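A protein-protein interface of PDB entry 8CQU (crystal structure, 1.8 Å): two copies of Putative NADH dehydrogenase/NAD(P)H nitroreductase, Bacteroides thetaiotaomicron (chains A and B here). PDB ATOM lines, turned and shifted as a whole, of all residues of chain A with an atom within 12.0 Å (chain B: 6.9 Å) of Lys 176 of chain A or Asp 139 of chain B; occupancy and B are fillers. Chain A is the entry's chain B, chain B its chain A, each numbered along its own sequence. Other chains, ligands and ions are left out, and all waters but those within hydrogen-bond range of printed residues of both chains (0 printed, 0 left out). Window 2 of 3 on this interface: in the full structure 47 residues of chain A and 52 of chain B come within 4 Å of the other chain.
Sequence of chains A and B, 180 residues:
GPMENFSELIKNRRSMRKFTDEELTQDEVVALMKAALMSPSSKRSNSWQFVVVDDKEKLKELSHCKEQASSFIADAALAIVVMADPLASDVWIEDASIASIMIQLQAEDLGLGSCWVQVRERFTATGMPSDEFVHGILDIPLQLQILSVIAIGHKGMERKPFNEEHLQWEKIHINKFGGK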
ATOM      1  N   TRP A 169     -17.755 -32.355  -9.006  1.00  0.00           N
ATOM      2  CA  TRP A 169     -17.077 -31.435  -9.912  1.00  0.00           C
ATOM      3  C   TRP A 169     -16.332 -30.295  -9.241  1.00  0.00           C
ATOM      4  O   TRP A 169     -15.445 -29.729  -9.886  1.00  0.00           O
ATOM      5  CB  TRP A 169     -18.019 -30.902 -10.987  1.00  0.00           C
ATOM      6  CG  TRP A 169     -18.380 -31.989 -11.953  1.00  0.00           C
ATOM      7  CD1 TRP A 169     -19.562 -32.653 -12.016  1.00  0.00           C
ATOM      8  CD2 TRP A 169     -17.587 -32.475 -13.041  1.00  0.00           C
ATOM      9  NE1 TRP A 169     -19.514 -33.590 -13.010  1.00  0.00           N
ATOM     10  CE2 TRP A 169     -18.329 -33.502 -13.661  1.00  0.00           C
ATOM     11  CE3 TRP A 169     -16.305 -32.174 -13.542  1.00  0.00           C
ATOM     12  CZ2 TRP A 169     -17.857 -34.217 -14.757  1.00  0.00           C
ATOM     13  CZ3 TRP A 169     -15.808 -32.908 -14.596  1.00  0.00           C
ATOM     14  CH2 TRP A 169     -16.582 -33.901 -15.205  1.00  0.00           C
ATOM     15  N   GLU A 170     -16.723 -29.943  -8.022  1.00  0.00           N
ATOM     16  CA  GLU A 170     -16.099 -28.884  -7.253  1.00  0.00           C
ATOM     17  C   GLU A 170     -14.654 -29.221  -6.932  1.00  0.00           C
ATOM     18  O   GLU A 170     -13.909 -28.280  -6.684  1.00  0.00           O
ATOM     19  CB  GLU A 170     -16.889 -28.506  -5.980  1.00  0.00           C
ATOM     20  CG  GLU A 170     -16.916 -29.576  -4.887  1.00  0.00           C
ATOM     21  CD  GLU A 170     -17.981 -30.658  -5.035  1.00  0.00           C
ATOM     22  OE1 GLU A 170     -18.089 -31.426  -4.061  1.00  0.00           O
ATOM     23  OE2 GLU A 170     -18.683 -30.736  -6.107  1.00  0.00           O
ATOM     24  N   LYS A 171     -14.275 -30.511  -7.077  1.00  0.00           N
ATOM     25  CA  LYS A 171     -12.894 -30.905  -6.867  1.00  0.00           C
ATOM     26  C   LYS A 171     -11.976 -30.720  -8.087  1.00  0.00           C
ATOM     27  O   LYS A 171     -10.819 -31.025  -7.940  1.00  0.00           O
ATOM     28  CB  LYS A 171     -12.891 -32.290  -6.266  1.00  0.00           C
ATOM     29  CG  LYS A 171     -13.501 -32.326  -4.858  1.00  0.00           C
ATOM     30  CD  LYS A 171     -13.818 -33.712  -4.408  1.00  0.00           C
ATOM     31  CE  LYS A 171     -14.026 -33.809  -2.915  1.00  0.00           C
ATOM     32  NZ  LYS A 171     -12.818 -33.387  -2.181  1.00  0.00           N
ATOM     33  N   ILE A 172     -12.501 -30.291  -9.230  1.00  0.00           N
ATOM     34  CA  ILE A 172     -11.802 -30.057 -10.484  1.00  0.00           C
ATOM     35  C   ILE A 172     -11.480 -28.586 -10.625  1.00  0.00           C
ATOM     36  O   ILE A 172     -12.384 -27.750 -10.572  1.00  0.00           O
ATOM     37  CB  ILE A 172     -12.613 -30.582 -11.678  1.00  0.00           C
ATOM     38  CG1 ILE A 172     -12.882 -32.079 -11.580  1.00  0.00           C
ATOM     39  CG2 ILE A 172     -12.029 -30.217 -13.050  1.00  0.00           C
ATOM     40  CD1 ILE A 172     -11.669 -32.915 -11.575  1.00  0.00           C
ATOM     41  N   HIS A 173     -10.167 -28.287 -10.765  1.00  0.00           N
ATOM     42  CA  HIS A 173      -9.700 -26.920 -10.997  1.00  0.00           C
ATOM     43  C   HIS A 173      -9.018 -26.865 -12.352  1.00  0.00           C
ATOM     44  O   HIS A 173      -8.280 -27.780 -12.636  1.00  0.00           O
ATOM     45  CB  HIS A 173      -8.675 -26.603  -9.918  1.00  0.00           C
ATOM     46  CG  HIS A 173      -9.226 -26.770  -8.578  1.00  0.00           C
ATOM     47  ND1 HIS A 173      -9.919 -25.762  -7.929  1.00  0.00           N
ATOM     48  CD2 HIS A 173      -9.357 -27.856  -7.816  1.00  0.00           C
ATOM     49  CE1 HIS A 173     -10.336 -26.229  -6.779  1.00  0.00           C
ATOM     50  NE2 HIS A 173      -9.972 -27.490  -6.685  1.00  0.00           N
ATOM     51  N   ILE A 174      -9.195 -25.778 -13.131  1.00  0.00           N
ATOM     52  CA  ILE A 174      -8.652 -25.665 -14.445  1.00  0.00           C
ATOM     53  C   ILE A 174      -7.443 -24.726 -14.384  1.00  0.00           C
ATOM     54  O   ILE A 174      -7.588 -23.551 -14.088  1.00  0.00           O
ATOM     55  CB  ILE A 174      -9.698 -25.150 -15.467  1.00  0.00           C
ATOM     56  CG1 ILE A 174     -11.036 -25.914 -15.384  1.00  0.00           C
ATOM     57  CG2 ILE A 174      -9.144 -25.179 -16.900  1.00  0.00           C
ATOM     58  CD1 ILE A 174     -10.913 -27.370 -15.718  1.00  0.00           C
ATOM     59  N   ASN A 175      -6.263 -25.260 -14.696  1.00  0.00           N
ATOM     60  CA  ASN A 175      -5.013 -24.530 -14.903  1.00  0.00           C
ATOM     61  C   ASN A 175      -4.421 -23.945 -13.620  1.00  0.00           C
ATOM     62  O   ASN A 175      -3.220 -23.705 -13.603  1.00  0.00           O
ATOM     63  CB  ASN A 175      -5.061 -23.478 -16.030  1.00  0.00           C
ATOM     64  CG  ASN A 175      -5.159 -24.084 -17.409  1.00  0.00           C
ATOM     65  OD1 ASN A 175      -5.965 -23.665 -18.270  1.00  0.00           O
ATOM     66  ND2 ASN A 175      -4.315 -25.082 -17.622  1.00  0.00           N
ATOM     67  N   LYS A 176      -5.233 -23.620 -12.606  1.00  0.00           N
ATOM     68  CA  LYS A 176      -4.695 -23.390 -11.287  1.00  0.00           C
ATOM     69  C   LYS A 176      -5.781 -23.620 -10.260  1.00  0.00           C
ATOM     70  O   LYS A 176      -6.970 -23.575 -10.585  1.00  0.00           O
ATOM     71  CB  LYS A 176      -4.201 -21.951 -11.150  1.00  0.00           C
ATOM     72  CG  LYS A 176      -5.213 -20.898 -11.412  1.00  0.00           C
ATOM     73  CD  LYS A 176      -4.641 -19.515 -11.213  1.00  0.00           C
ATOM     74  CE  LYS A 176      -4.207 -19.304  -9.788  1.00  0.00           C
ATOM     75  NZ  LYS A 176      -4.084 -17.884  -9.482  1.00  0.00           N
ATOM     76  N   PHE A 177      -5.343 -23.727  -9.027  1.00  0.00           N
ATOM     77  CA  PHE A 177      -6.266 -23.956  -7.951  1.00  0.00           C
ATOM     78  C   PHE A 177      -7.212 -22.772  -7.827  1.00  0.00           C
ATOM     79  O   PHE A 177      -6.770 -21.625  -7.822  1.00  0.00           O
ATOM     80  CB  PHE A 177      -5.550 -24.159  -6.642  1.00  0.00           C
ATOM     81  CG  PHE A 177      -6.462 -24.754  -5.620  1.00  0.00           C
ATOM     82  CD1 PHE A 177      -6.645 -26.138  -5.569  1.00  0.00           C
ATOM     83  CD2 PHE A 177      -7.169 -23.939  -4.755  1.00  0.00           C
ATOM     84  CE1 PHE A 177      -7.419 -26.705  -4.573  1.00  0.00           C
ATOM     85  CE2 PHE A 177      -7.996 -24.518  -3.790  1.00  0.00           C
ATOM     86  CZ  PHE A 177      -8.123 -25.882  -3.704  1.00  0.00           C
ATOM     87  N   GLY A 178      -8.505 -23.082  -7.902  1.00  0.00           N
ATOM     88  CA  GLY A 178      -9.580 -22.103  -7.855  1.00  0.00           C
ATOM     89  C   GLY A 178      -9.883 -21.442  -9.181  1.00  0.00           C
ATOM     90  O   GLY A 178     -10.705 -20.531  -9.197  1.00  0.00           O
ATOM     91  N   GLY A 179      -9.165 -21.790 -10.259  1.00  0.00           N
ATOM     92  CA  GLY A 179      -9.436 -21.229 -11.569  1.00  0.00           C
ATOM     93  C   GLY A 179      -8.761 -19.872 -11.753  1.00  0.00           C
ATOM     94  O   GLY A 179      -8.430 -19.204 -10.772  1.00  0.00           O
ATOM     95  N   LYS A 180      -8.485 -19.541 -13.020  1.00  0.00           N
ATOM     96  CA  LYS A 180      -8.338 -18.191 -13.558  1.00  0.00           C
ATOM     97  C   LYS A 180      -7.441 -18.245 -14.807  1.00  0.00           C
ATOM     98  O   LYS A 180      -7.697 -17.432 -15.706  1.00  0.00           O
ATOM     99  CB  LYS A 180      -7.795 -17.157 -12.565  1.00  0.00           C
ATOM    100  CG  LYS A 180      -8.138 -15.713 -12.890  1.00  0.00           C
ATOM    101  CD  LYS A 180      -6.961 -14.782 -12.647  1.00  0.00           C
ATOM    102  CE  LYS A 180      -6.428 -14.825 -11.233  1.00  0.00           C
ATOM    103  NZ  LYS A 180      -5.606 -13.623 -10.946  1.00  0.00           N
ATOM    104  OXT LYS A 180      -6.504 -19.064 -14.860  1.00  0.00           O
ATOM    105  N   PHE B  50      -8.027 -32.060  -7.860  1.00  0.00           N
ATOM    106  CA  PHE B  50      -7.330 -32.192  -9.135  1.00  0.00           C
ATOM    107  C   PHE B  50      -7.165 -30.827  -9.764  1.00  0.00           C
ATOM    108  O   PHE B  50      -8.155 -30.121  -9.884  1.00  0.00           O
ATOM    109  CB  PHE B  50      -8.106 -33.090 -10.089  1.00  0.00           C
ATOM    110  CG  PHE B  50      -8.401 -34.434  -9.510  1.00  0.00           C
ATOM    111  CD1 PHE B  50      -7.445 -35.441  -9.541  1.00  0.00           C
ATOM    112  CD2 PHE B  50      -9.633 -34.667  -8.860  1.00  0.00           C
ATOM    113  CE1 PHE B  50      -7.717 -36.645  -8.925  1.00  0.00           C
ATOM    114  CE2 PHE B  50      -9.907 -35.904  -8.316  1.00  0.00           C
ATOM    115  CZ  PHE B  50      -8.958 -36.876  -8.349  1.00  0.00           C
ATOM    116  N   VAL B  51      -5.934 -30.524 -10.210  1.00  0.00           N
ATOM    117  CA  VAL B  51      -5.717 -29.403 -11.100  1.00  0.00           C
ATOM    118  C   VAL B  51      -5.414 -29.959 -12.505  1.00  0.00           C
ATOM    119  O   VAL B  51      -4.435 -30.657 -12.731  1.00  0.00           O
ATOM    120  CB  VAL B  51      -4.637 -28.421 -10.613  1.00  0.00           C
ATOM    121  CG1 VAL B  51      -4.547 -27.253 -11.590  1.00  0.00           C
ATOM    122  CG2 VAL B  51      -4.869 -27.920  -9.190  1.00  0.00           C
ATOM    123  N   VAL B  52      -6.298 -29.649 -13.489  1.00  0.00           N
ATOM    124  CA  VAL B  52      -6.197 -30.072 -14.857  1.00  0.00           C
ATOM    125  C   VAL B  52      -5.584 -28.944 -15.686  1.00  0.00           C
ATOM    126  O   VAL B  52      -6.143 -27.826 -15.740  1.00  0.00           O
ATOM    127  CB  VAL B  52      -7.601 -30.400 -15.392  1.00  0.00           C
ATOM    128  CG1 VAL B  52      -7.454 -30.824 -16.853  1.00  0.00           C
ATOM    129  CG2 VAL B  52      -8.313 -31.408 -14.532  1.00  0.00           C
ATOM    130  N   VAL B  53      -4.382 -29.206 -16.203  1.00  0.00           N
ATOM    131  CA  VAL B  53      -3.534 -28.181 -16.828  1.00  0.00           C
ATOM    132  C   VAL B  53      -3.443 -28.444 -18.308  1.00  0.00           C
ATOM    133  O   VAL B  53      -2.984 -29.534 -18.710  1.00  0.00           O
ATOM    134  CB  VAL B  53      -2.155 -28.137 -16.175  1.00  0.00           C
ATOM    135  CG1 VAL B  53      -1.278 -27.029 -16.788  1.00  0.00           C
ATOM    136  CG2 VAL B  53      -2.253 -27.956 -14.686  1.00  0.00           C
ATOM    137  N   LYS B  58       2.288 -23.295 -18.327  1.00  0.00           N
ATOM    138  CA  LYS B  58       2.214 -24.020 -17.056  1.00  0.00           C
ATOM    139  C   LYS B  58       2.768 -25.446 -17.185  1.00  0.00           C
ATOM    140  O   LYS B  58       3.452 -25.940 -16.279  1.00  0.00           O
ATOM    141  CB  LYS B  58       0.781 -23.955 -16.502  1.00  0.00           C
ATOM    142  CG  LYS B  58       0.379 -22.593 -15.938  1.00  0.00           C
ATOM    143  CD  LYS B  58       0.981 -22.364 -14.529  1.00  0.00           C
ATOM    144  CE  LYS B  58       0.951 -20.946 -13.992  1.00  0.00           C
ATOM    145  NZ  LYS B  58       2.090 -20.651 -13.068  1.00  0.00           N
ATOM    146  N   VAL B 134       5.346 -27.462  -6.913  1.00  0.00           N
ATOM    147  CA  VAL B 134       4.102 -27.534  -7.679  1.00  0.00           C
ATOM    148  C   VAL B 134       3.058 -26.614  -7.017  1.00  0.00           C
ATOM    149  O   VAL B 134       2.262 -25.929  -7.712  1.00  0.00           O
ATOM    150  CB  VAL B 134       3.661 -29.005  -7.846  1.00  0.00           C
ATOM    151  CG1 VAL B 134       2.259 -29.116  -8.472  1.00  0.00           C
ATOM    152  CG2 VAL B 134       4.688 -29.795  -8.679  1.00  0.00           C
ATOM    153  N   HIS B 135       3.031 -26.579  -5.691  1.00  0.00           N
ATOM    154  CA  HIS B 135       2.184 -25.696  -4.911  1.00  0.00           C
ATOM    155  C   HIS B 135       2.361 -24.262  -5.434  1.00  0.00           C
ATOM    156  O   HIS B 135       1.360 -23.561  -5.602  1.00  0.00           O
ATOM    157  CB  HIS B 135       2.493 -25.721  -3.402  1.00  0.00           C
ATOM    158  CG  HIS B 135       1.844 -26.835  -2.649  1.00  0.00           C
ATOM    159  ND1 HIS B 135       0.650 -26.619  -2.030  1.00  0.00           N
ATOM    160  CD2 HIS B 135       2.112 -28.101  -2.409  1.00  0.00           C
ATOM    161  CE1 HIS B 135       0.263 -27.741  -1.450  1.00  0.00           C
ATOM    162  NE2 HIS B 135       1.137 -28.638  -1.664  1.00  0.00           N
ATOM    163  N   GLY B 136       3.632 -23.822  -5.586  1.00  0.00           N
ATOM    164  CA  GLY B 136       3.957 -22.502  -6.106  1.00  0.00           C
ATOM    165  C   GLY B 136       3.497 -22.265  -7.540  1.00  0.00           C
ATOM    166  O   GLY B 136       2.989 -21.176  -7.828  1.00  0.00           O
ATOM    167  N   ILE B 137       3.673 -23.249  -8.444  1.00  0.00           N
ATOM    168  CA  ILE B 137       3.249 -23.110  -9.851  1.00  0.00           C
ATOM    169  C   ILE B 137       1.735 -22.893  -9.959  1.00  0.00           C
ATOM    170  O   ILE B 137       1.312 -22.098 -10.781  1.00  0.00           O
ATOM    171  CB  ILE B 137       3.674 -24.331 -10.729  1.00  0.00           C
ATOM    172  CG1 ILE B 137       5.175 -24.627 -10.691  1.00  0.00           C
ATOM    173  CG2 ILE B 137       3.235 -24.197 -12.181  1.00  0.00           C
ATOM    174  CD1 ILE B 137       6.015 -23.367 -10.740  1.00  0.00           C
ATOM    175  N   LEU B 138       0.921 -23.678  -9.209  1.00  0.00           N
ATOM    176  CA  LEU B 138      -0.511 -23.747  -9.439  1.00  0.00           C
ATOM    177  C   LEU B 138      -1.365 -23.101  -8.328  1.00  0.00           C
ATOM    178  O   LEU B 138      -2.579 -23.302  -8.310  1.00  0.00           O
ATOM    179  CB  LEU B 138      -0.814 -25.220  -9.594  1.00  0.00           C
ATOM    180  CG  LEU B 138      -0.173 -25.946 -10.751  1.00  0.00           C
ATOM    181  CD1 LEU B 138      -0.666 -27.405 -10.694  1.00  0.00           C
ATOM    182  CD2 LEU B 138      -0.550 -25.259 -12.072  1.00  0.00           C
ATOM    183  N   ASP B 139      -0.743 -22.320  -7.423  1.00  0.00           N
ATOM    184  CA  ASP B 139      -1.400 -21.664  -6.295  1.00  0.00           C
ATOM    185  C   ASP B 139      -2.257 -22.610  -5.438  1.00  0.00           C
ATOM    186  O   ASP B 139      -3.381 -22.288  -5.065  1.00  0.00           O
ATOM    187  CB  ASP B 139      -2.214 -20.481  -6.820  1.00  0.00           C
ATOM    188  CG  ASP B 139      -2.576 -19.434  -5.776  1.00  0.00           C
ATOM    189  OD1 ASP B 139      -2.019 -19.471  -4.632  1.00  0.00           O
ATOM    190  OD2 ASP B 139      -3.432 -18.587  -6.107  1.00  0.00           O
ATOM    191  N   ILE B 140      -1.706 -23.760  -5.080  1.00  0.00           N
ATOM    192  CA  ILE B 140      -2.451 -24.775  -4.337  1.00  0.00           C
ATOM    193  C   ILE B 140      -2.242 -24.500  -2.841  1.00  0.00           C
ATOM    194  O   ILE B 140      -1.100 -24.239  -2.426  1.00  0.00           O
ATOM    195  CB  ILE B 140      -1.949 -26.165  -4.715  1.00  0.00           C
ATOM    196  CG1 ILE B 140      -2.152 -26.464  -6.218  1.00  0.00           C
ATOM    197  CG2 ILE B 140      -2.506 -27.237  -3.773  1.00  0.00           C
ATOM    198  CD1 ILE B 140      -1.307 -27.597  -6.743  1.00  0.00           C
ATOM    199  N   PRO B 141      -3.286 -24.578  -1.990  1.00  0.00           N
ATOM    200  CA  PRO B 141      -3.105 -24.304  -0.564  1.00  0.00           C
ATOM    201  C   PRO B 141      -2.165 -25.349   0.051  1.00  0.00           C
ATOM    202  O   PRO B 141      -2.210 -26.514  -0.331  1.00  0.00           O
ATOM    203  CB  PRO B 141      -4.511 -24.407   0.047  1.00  0.00           C
ATOM    204  CG  PRO B 141      -5.480 -24.489  -1.106  1.00  0.00           C
ATOM    205  CD  PRO B 141      -4.680 -24.844  -2.343  1.00  0.00           C
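The backbone NH (N) of Phe 50 of chain B is in hydrogen-bond range of the backbone carbonyl oxygen (O) of Lys 171 of chain A, 3.0 Å away.
N of Phe 177 of chain A is in hydrogen-bond range of O of Leu 138 of chain B, at 2.9 Å.
The backbone NH of Val 52 of chain B lies within hydrogen-bond range of the backbone carbonyl oxygen of His 173 of chain A (2.9 Å).
The side-chain carboxylate of Asp 139 of chain B lies within salt-bridge range of the side-chain amino group of Lys 176 of chain A, 3.5 Å away.
O of Phe 50 of chain B sits at hydrogen-bond distance from N of His 173 of chain A, at 2.9 Å.
O of Val 52 of chain B sits at hydrogen-bond distance from N of Asn 175 of chain A (2.8 Å).
O of Pro 141 of chain B lies close to ND1 of His 135 of chain B (3.3 Å).
A ring nitrogen (ND1) of His 173 of chain A sits at hydrogen-bond distance from the backbone NH (N) of Gly 178 of chain A (3.0 Å).
O of Ile 140 of chain B is in hydrogen-bond range of ND1 of His 135 of chain B (3.0 Å).
Among the printed residues, merely in contact across the chains: Phe 177 of chain A with Asp 139 of chain B (3.3 Å), Asn 175 of chain A with Val 53 of chain B (3.3 Å), His 173 of chain A with Val 51 of chain B (3.4 Å), Asn 175 of chain A with Leu 138 of chain B (3.4 Å), Lys 176 of chain A with Leu 138 of chain B (3.5 Å), Ile 174 of chain A with Val 52 of chain B (3.6 Å), Phe 177 of chain A with Pro 141 of chain B (3.6 Å), Ile 172 of chain A with Phe 50 of chain B (3.7 Å), Lys 176 of chain A with Val 51 of chain B (3.8 Å), Asn 175 of chain A with Val 51 of chain B (3.9 Å) and Phe 177 of chain A with Ile 140 of chain B (3.9 Å).
Printed residues of chain B within 4 Å of Ile 174 of chain A: Val 52.
Of the printed residues of chain B, Asn 175 of chain A touches Val 51, Val 52, Val 53 and Leu 138.
Lys 176 of chain A touches three residues of chain B.
Printed residues of chain A within 4 Å of Val 51 of chain B: His 173 (3.4 Å), Asn 175 (3.9 Å) and Lys 176 (3.8 Å).
No residue of chain A comes within 4 Å of Gly 136 of chain B.
No residue of chain A comes within 4 Å of Ile 137 of chain B.
Leu 138 of chain B touches three residues of chain A.
Of chain A, only Lys 176 (3.5 Å) and Phe 177 (3.3 Å) come within 4 Å of Asp 139 of chain B.
Pro 141 of chain B touches just one residue of chain A: Phe 177.
Of the 12 printed residues of chain A, 7 touch a printed residue of chain B.
Hydrophobic or aromatic side chains of chain A that line the printed part of chain B: Ile 172, His 173 and Phe 177.
Of the 13 printed residues of chain B, 8 touch a printed residue of chain A.
Hydrophobic or aromatic side chains of chain B within 4 Å of the printed part of chain A: Phe 50, Val 51, Val 52, Val 53, Leu 138 and Pro 141.
Along chain B the printed residues that touch a printed residue of chain A span positions 50 to 141.
Among the printed residues, Asp or Glu carboxylates within 4 Å of a Lys or Arg side-chain nitrogen of the other chain: Lys 176 of chain A with Asp 139 of chain B.
No position is printed for both chains.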
